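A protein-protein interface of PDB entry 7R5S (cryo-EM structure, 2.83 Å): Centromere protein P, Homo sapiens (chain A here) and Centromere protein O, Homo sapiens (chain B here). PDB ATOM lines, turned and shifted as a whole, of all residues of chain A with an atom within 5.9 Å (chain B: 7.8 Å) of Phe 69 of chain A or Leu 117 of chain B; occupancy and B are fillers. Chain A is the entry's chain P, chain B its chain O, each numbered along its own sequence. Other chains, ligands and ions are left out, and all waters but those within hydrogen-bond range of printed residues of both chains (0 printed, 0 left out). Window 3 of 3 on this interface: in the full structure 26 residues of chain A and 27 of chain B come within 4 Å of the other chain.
OH of Tyr 108 of chain B is in hydrogen-bond range of O of Leu 70 of chain A, 3.5 Å away.
N of Cys 123 of chain B lies within hydrogen-bond range of O of Lys 116 of chain B, 2.9 Å away. The side-chain hydroxyl (OG1) of Thr 74 of chain A sits at hydrogen-bond distance from the backbone carbonyl oxygen (O) of Leu 70 of chain A (3.4 Å).
Glu 66 of chain A touches Lys 116 of chain B. Glu 66 of chain A touches Leu 117 of chain B. Phe 69 of chain A touches Leu 117 of chain B (CE2 to CD2, 3.6 Å). CZ of Phe 69 of chain A touches CG2 of Val 122 of chain B, 3.6 Å away. N of Gly 115 of chain B touches CD1 of Leu 70 of chain A (3.7 Å). OH of Tyr 108 of chain B touches CA of Ser 71 of chain A (3.6 Å). Tyr 108 of chain B touches Thr 74 of chain A (OH to CB, 3.2 Å).
Printed residues of chain B within 4 Å of Glu 66 of chain A: Lys 116 (3.9 Å) and Leu 117 (3.6 Å). Leu 67 of chain A touches none of the printed residues of chain B. No residue of chain B comes within 4 Å of Ser 68 of chain A. Phe 69 of chain A touches just these residues of chain B: Leu 117 (3.6 Å) and Val 122 (3.6 Å). Printed residues of chain B within 4 Å of Ser 71 of chain A: Tyr 108 (3.6 Å). Leu 73 of chain A touches none of the printed residues of chain B. Of chain A, only Glu 66 and Phe 69 come within 4 Å of Leu 117 of chain B. The nearest residue of chain A that does not touch Leu 117 of chain B is Ser 65 of chain A (5.5 Å). The nearest printed residue of chain B that does not touch Leu 70 of chain A is Lys 116 of chain B (5.4 Å).
Hydrophobic or aromatic side chains of chain B within 4 Å of the printed part of chain A: Tyr 108, Leu 117 and Val 122. Along chain B the printed residues that touch a printed residue of chain A span positions 108 to 122. Of the 11 printed residues of chain A, 5 touch a printed residue of chain B. Printed residues of chain A that touch a printed residue of chain B: Glu 66, Phe 69, Leu 70, Ser 71 and Thr 74. Among the printed residues, 8 pairs touch across the chains.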
ATOM      1  N   GLU A  64      -2.063 -34.315   8.699  1.00  0.00           N
ATOM      2  CA  GLU A  64      -0.805 -34.271   7.959  1.00  0.00           C
ATOM      3  C   GLU A  64      -0.331 -32.835   7.762  1.00  0.00           C
ATOM      4  O   GLU A  64       0.867 -32.547   7.887  1.00  0.00           O
ATOM      5  CB  GLU A  64      -0.963 -34.976   6.612  1.00  0.00           C
ATOM      6  CG  GLU A  64      -1.100 -36.487   6.713  1.00  0.00           C
ATOM      7  CD  GLU A  64       0.202 -37.170   7.085  1.00  0.00           C
ATOM      8  OE1 GLU A  64       1.273 -36.556   6.901  1.00  0.00           O
ATOM      9  OE2 GLU A  64       0.153 -38.324   7.562  1.00  0.00           O
ATOM     10  N   SER A  65      -1.257 -31.919   7.464  1.00  0.00           N
ATOM     11  CA  SER A  65      -0.884 -30.519   7.300  1.00  0.00           C
ATOM     12  C   SER A  65      -0.369 -29.929   8.606  1.00  0.00           C
ATOM     13  O   SER A  65       0.620 -29.187   8.613  1.00  0.00           O
ATOM     14  CB  SER A  65      -2.075 -29.715   6.780  1.00  0.00           C
ATOM     15  OG  SER A  65      -2.888 -29.260   7.848  1.00  0.00           O
ATOM     16  N   GLU A  66      -1.022 -30.253   9.726  1.00  0.00           N
ATOM     17  CA  GLU A  66      -0.561 -29.760  11.019  1.00  0.00           C
ATOM     18  C   GLU A  66       0.807 -30.333  11.371  1.00  0.00           C
ATOM     19  O   GLU A  66       1.660 -29.628  11.924  1.00  0.00           O
ATOM     20  CB  GLU A  66      -1.582 -30.101  12.104  1.00  0.00           C
ATOM     21  CG  GLU A  66      -1.190 -29.637  13.496  1.00  0.00           C
ATOM     22  CD  GLU A  66      -2.264 -29.917  14.528  1.00  0.00           C
ATOM     23  OE1 GLU A  66      -3.415 -30.192  14.128  1.00  0.00           O
ATOM     24  OE2 GLU A  66      -1.959 -29.862  15.737  1.00  0.00           O
ATOM     25  N   LEU A  67       1.035 -31.609  11.052  1.00  0.00           N
ATOM     26  CA  LEU A  67       2.336 -32.220  11.301  1.00  0.00           C
ATOM     27  C   LEU A  67       3.424 -31.525  10.492  1.00  0.00           C
ATOM     28  O   LEU A  67       4.496 -31.203  11.018  1.00  0.00           O
ATOM     29  CB  LEU A  67       2.279 -33.711  10.971  1.00  0.00           C
ATOM     30  CG  LEU A  67       3.268 -34.658  11.655  1.00  0.00           C
ATOM     31  CD1 LEU A  67       2.708 -36.070  11.662  1.00  0.00           C
ATOM     32  CD2 LEU A  67       4.629 -34.632  10.977  1.00  0.00           C
ATOM     33  N   SER A  68       3.163 -31.284   9.205  1.00  0.00           N
ATOM     34  CA  SER A  68       4.143 -30.594   8.371  1.00  0.00           C
ATOM     35  C   SER A  68       4.399 -29.178   8.874  1.00  0.00           C
ATOM     36  O   SER A  68       5.545 -28.712   8.881  1.00  0.00           O
ATOM     37  CB  SER A  68       3.669 -30.570   6.917  1.00  0.00           C
ATOM     38  OG  SER A  68       4.305 -29.531   6.193  1.00  0.00           O
ATOM     39  N   PHE A  69       3.342 -28.481   9.301  1.00  0.00           N
ATOM     40  CA  PHE A  69       3.497 -27.124   9.814  1.00  0.00           C
ATOM     41  C   PHE A  69       4.358 -27.108  11.070  1.00  0.00           C
ATOM     42  O   PHE A  69       5.265 -26.279  11.204  1.00  0.00           O
ATOM     43  CB  PHE A  69       2.122 -26.512  10.089  1.00  0.00           C
ATOM     44  CG  PHE A  69       2.137 -25.430  11.132  1.00  0.00           C
ATOM     45  CD1 PHE A  69       2.572 -24.153  10.820  1.00  0.00           C
ATOM     46  CD2 PHE A  69       1.703 -25.687  12.423  1.00  0.00           C
ATOM     47  CE1 PHE A  69       2.583 -23.156  11.774  1.00  0.00           C
ATOM     48  CE2 PHE A  69       1.713 -24.694  13.382  1.00  0.00           C
ATOM     49  CZ  PHE A  69       2.154 -23.427  13.057  1.00  0.00           C
ATOM     50  N   LEU A  70       4.085 -28.018  12.007  1.00  0.00           N
ATOM     51  CA  LEU A  70       4.891 -28.088  13.221  1.00  0.00           C
ATOM     52  C   LEU A  70       6.335 -28.451  12.899  1.00  0.00           C
ATOM     53  O   LEU A  70       7.270 -27.924  13.517  1.00  0.00           O
ATOM     54  CB  LEU A  70       4.286 -29.097  14.196  1.00  0.00           C
ATOM     55  CG  LEU A  70       4.885 -29.124  15.603  1.00  0.00           C
ATOM     56  CD1 LEU A  70       4.719 -27.775  16.282  1.00  0.00           C
ATOM     57  CD2 LEU A  70       4.249 -30.228  16.435  1.00  0.00           C
ATOM     58  N   SER A  71       6.538 -29.339  11.922  1.00  0.00           N
ATOM     59  CA  SER A  71       7.892 -29.753  11.567  1.00  0.00           C
ATOM     60  C   SER A  71       8.687 -28.602  10.966  1.00  0.00           C
ATOM     61  O   SER A  71       9.867 -28.422  11.289  1.00  0.00           O
ATOM     62  CB  SER A  71       7.841 -30.933  10.598  1.00  0.00           C
ATOM     63  OG  SER A  71       9.086 -31.609  10.553  1.00  0.00           O
ATOM     64  N   THR A  72       8.066 -27.810  10.090  1.00  0.00           N
ATOM     65  CA  THR A  72       8.785 -26.689   9.494  1.00  0.00           C
ATOM     66  C   THR A  72       8.867 -25.484  10.422  1.00  0.00           C
ATOM     67  O   THR A  72       9.707 -24.606  10.200  1.00  0.00           O
ATOM     68  CB  THR A  72       8.143 -26.266   8.171  1.00  0.00           C
ATOM     69  OG1 THR A  72       8.857 -25.147   7.631  1.00  0.00           O
ATOM     70  CG2 THR A  72       6.706 -25.860   8.386  1.00  0.00           C
ATOM     71  N   LEU A  73       8.020 -25.420  11.452  1.00  0.00           N
ATOM     72  CA  LEU A  73       8.121 -24.339  12.427  1.00  0.00           C
ATOM     73  C   LEU A  73       9.220 -24.612  13.444  1.00  0.00           C
ATOM     74  O   LEU A  73      10.098 -23.770  13.661  1.00  0.00           O
ATOM     75  CB  LEU A  73       6.778 -24.141  13.132  1.00  0.00           C
ATOM     76  CG  LEU A  73       6.783 -23.181  14.324  1.00  0.00           C
ATOM     77  CD1 LEU A  73       7.119 -21.767  13.876  1.00  0.00           C
ATOM     78  CD2 LEU A  73       5.446 -23.216  15.049  1.00  0.00           C
ATOM     79  N   THR A  74       9.188 -25.786  14.079  1.00  0.00           N
ATOM     80  CA  THR A  74      10.210 -26.114  15.067  1.00  0.00           C
ATOM     81  C   THR A  74      11.560 -26.360  14.405  1.00  0.00           C
ATOM     82  O   THR A  74      12.596 -25.904  14.905  1.00  0.00           O
ATOM     83  CB  THR A  74       9.779 -27.334  15.882  1.00  0.00           C
ATOM     84  OG1 THR A  74       8.568 -27.036  16.587  1.00  0.00           O
ATOM     85  CG2 THR A  74      10.857 -27.720  16.882  1.00  0.00           C
ATOM     86  N   TYR B 108       6.833 -36.174  19.207  1.00  0.00           N
ATOM     87  CA  TYR B 108       7.296 -34.814  18.954  1.00  0.00           C
ATOM     88  C   TYR B 108       7.176 -33.952  20.201  1.00  0.00           C
ATOM     89  O   TYR B 108       7.946 -33.003  20.378  1.00  0.00           O
ATOM     90  CB  TYR B 108       6.495 -34.195  17.808  1.00  0.00           C
ATOM     91  CG  TYR B 108       7.257 -33.168  17.009  1.00  0.00           C
ATOM     92  CD1 TYR B 108       7.877 -33.513  15.818  1.00  0.00           C
ATOM     93  CD2 TYR B 108       7.358 -31.854  17.443  1.00  0.00           C
ATOM     94  CE1 TYR B 108       8.574 -32.582  15.080  1.00  0.00           C
ATOM     95  CE2 TYR B 108       8.056 -30.913  16.713  1.00  0.00           C
ATOM     96  CZ  TYR B 108       8.662 -31.285  15.531  1.00  0.00           C
ATOM     97  OH  TYR B 108       9.359 -30.356  14.794  1.00  0.00           O
ATOM     98  N   GLY B 115       3.588 -27.862  19.799  1.00  0.00           N
ATOM     99  CA  GLY B 115       2.614 -26.872  19.370  1.00  0.00           C
ATOM    100  C   GLY B 115       1.346 -27.524  18.875  1.00  0.00           C
ATOM    101  O   GLY B 115       1.363 -28.641  18.347  1.00  0.00           O
ATOM    102  N   LYS B 116       0.232 -26.816  19.050  1.00  0.00           N
ATOM    103  CA  LYS B 116      -1.067 -27.289  18.588  1.00  0.00           C
ATOM    104  C   LYS B 116      -1.830 -26.142  17.944  1.00  0.00           C
ATOM    105  O   LYS B 116      -1.854 -25.027  18.471  1.00  0.00           O
ATOM    106  CB  LYS B 116      -1.896 -27.881  19.736  1.00  0.00           C
ATOM    107  CG  LYS B 116      -3.256 -28.404  19.298  1.00  0.00           C
ATOM    108  CD  LYS B 116      -4.060 -28.937  20.470  1.00  0.00           C
ATOM    109  CE  LYS B 116      -5.412 -29.461  20.015  1.00  0.00           C
ATOM    110  NZ  LYS B 116      -6.212 -29.997  21.148  1.00  0.00           N
ATOM    111  N   LEU B 117      -2.461 -26.425  16.807  1.00  0.00           N
ATOM    112  CA  LEU B 117      -3.250 -25.422  16.104  1.00  0.00           C
ATOM    113  C   LEU B 117      -4.614 -25.267  16.766  1.00  0.00           C
ATOM    114  O   LEU B 117      -5.334 -26.250  16.964  1.00  0.00           O
ATOM    115  CB  LEU B 117      -3.417 -25.810  14.636  1.00  0.00           C
ATOM    116  CG  LEU B 117      -2.194 -25.627  13.737  1.00  0.00           C
ATOM    117  CD1 LEU B 117      -2.439 -26.242  12.369  1.00  0.00           C
ATOM    118  CD2 LEU B 117      -1.848 -24.154  13.608  1.00  0.00           C
ATOM    119  N   THR B 118      -4.965 -24.032  17.108  1.00  0.00           N
ATOM    120  CA  THR B 118      -6.258 -23.711  17.694  1.00  0.00           C
ATOM    121  C   THR B 118      -6.981 -22.705  16.797  1.00  0.00           C
ATOM    122  O   THR B 118      -6.537 -22.397  15.688  1.00  0.00           O
ATOM    123  CB  THR B 118      -6.097 -23.184  19.124  1.00  0.00           C
ATOM    124  OG1 THR B 118      -7.376 -22.794  19.638  1.00  0.00           O
ATOM    125  CG2 THR B 118      -5.165 -21.985  19.155  1.00  0.00           C
ATOM    126  N   SER B 119      -8.113 -22.197  17.288  1.00  0.00           N
ATOM    127  CA  SER B 119      -8.924 -21.277  16.495  1.00  0.00           C
ATOM    128  C   SER B 119      -8.185 -19.969  16.237  1.00  0.00           C
ATOM    129  O   SER B 119      -8.065 -19.527  15.088  1.00  0.00           O
ATOM    130  CB  SER B 119     -10.255 -21.015  17.199  1.00  0.00           C
ATOM    131  OG  SER B 119     -10.142 -19.947  18.123  1.00  0.00           O
ATOM    132  N   ARG B 120      -7.684 -19.332  17.297  1.00  0.00           N
ATOM    133  CA  ARG B 120      -7.025 -18.040  17.137  1.00  0.00           C
ATOM    134  C   ARG B 120      -5.650 -18.178  16.495  1.00  0.00           C
ATOM    135  O   ARG B 120      -5.173 -17.236  15.852  1.00  0.00           O
ATOM    136  CB  ARG B 120      -6.904 -17.338  18.490  1.00  0.00           C
ATOM    137  CG  ARG B 120      -8.233 -17.039  19.158  1.00  0.00           C
ATOM    138  CD  ARG B 120      -8.048 -16.771  20.641  1.00  0.00           C
ATOM    139  NE  ARG B 120      -7.414 -17.896  21.321  1.00  0.00           N
ATOM    140  CZ  ARG B 120      -8.074 -18.942  21.808  1.00  0.00           C
ATOM    141  NH1 ARG B 120      -9.393 -19.009  21.692  1.00  0.00           N
ATOM    142  NH2 ARG B 120      -7.415 -19.921  22.412  1.00  0.00           N
ATOM    143  N   GLY B 121      -5.003 -19.329  16.651  1.00  0.00           N
ATOM    144  CA  GLY B 121      -3.655 -19.497  16.146  1.00  0.00           C
ATOM    145  C   GLY B 121      -2.983 -20.772  16.606  1.00  0.00           C
ATOM    146  O   GLY B 121      -3.540 -21.864  16.463  1.00  0.00           O
ATOM    147  N   VAL B 122      -1.770 -20.649  17.139  1.00  0.00           N
ATOM    148  CA  VAL B 122      -0.998 -21.783  17.629  1.00  0.00           C
ATOM    149  C   VAL B 122      -0.765 -21.607  19.122  1.00  0.00           C
ATOM    150  O   VAL B 122      -0.546 -20.489  19.600  1.00  0.00           O
ATOM    151  CB  VAL B 122       0.346 -21.923  16.885  1.00  0.00           C
ATOM    152  CG1 VAL B 122       0.934 -23.309  17.100  1.00  0.00           C
ATOM    153  CG2 VAL B 122       0.167 -21.635  15.404  1.00  0.00           C
ATOM    154  N   CYS B 123      -0.816 -22.716  19.857  1.00  0.00           N
ATOM    155  CA  CYS B 123      -0.498 -22.749  21.279  1.00  0.00           C
ATOM    156  C   CYS B 123       0.753 -23.595  21.458  1.00  0.00           C
ATOM    157  O   CYS B 123       0.778 -24.761  21.048  1.00  0.00           O
ATOM    158  CB  CYS B 123      -1.662 -23.317  22.094  1.00  0.00           C
ATOM    159  SG  CYS B 123      -1.667 -22.829  23.833  1.00  0.00           S
ATOM    160  N   VAL B 124       1.785 -23.006  22.058  1.00  0.00           N
ATOM    161  CA  VAL B 124       3.092 -23.634  22.198  1.00  0.00           C
ATOM    162  C   VAL B 124       3.288 -24.051  23.647  1.00  0.00           C
ATOM    163  O   VAL B 124       2.873 -23.343  24.573  1.00  0.00           O
ATOM    164  CB  VAL B 124       4.217 -22.683  21.740  1.00  0.00           C
ATOM    165  CG1 VAL B 124       5.548 -23.416  21.671  1.00  0.00           C
ATOM    166  CG2 VAL B 124       3.871 -22.065  20.395  1.00  0.00           C
ATOM    167  N   ILE B 144      -2.108 -15.382  14.921  1.00  0.00           N
ATOM    168  CA  ILE B 144      -1.415 -15.327  13.638  1.00  0.00           C
ATOM    169  C   ILE B 144      -1.685 -14.043  12.859  1.00  0.00           C
ATOM    170  O   ILE B 144      -0.851 -13.647  12.033  1.00  0.00           O
ATOM    171  CB  ILE B 144      -1.785 -16.547  12.773  1.00  0.00           C
ATOM    172  CG1 ILE B 144      -1.805 -17.817  13.623  1.00  0.00           C
ATOM    173  CG2 ILE B 144      -0.797 -16.719  11.629  1.00  0.00           C
ATOM    174  CD1 ILE B 144      -0.469 -18.163  14.242  1.00  0.00           C
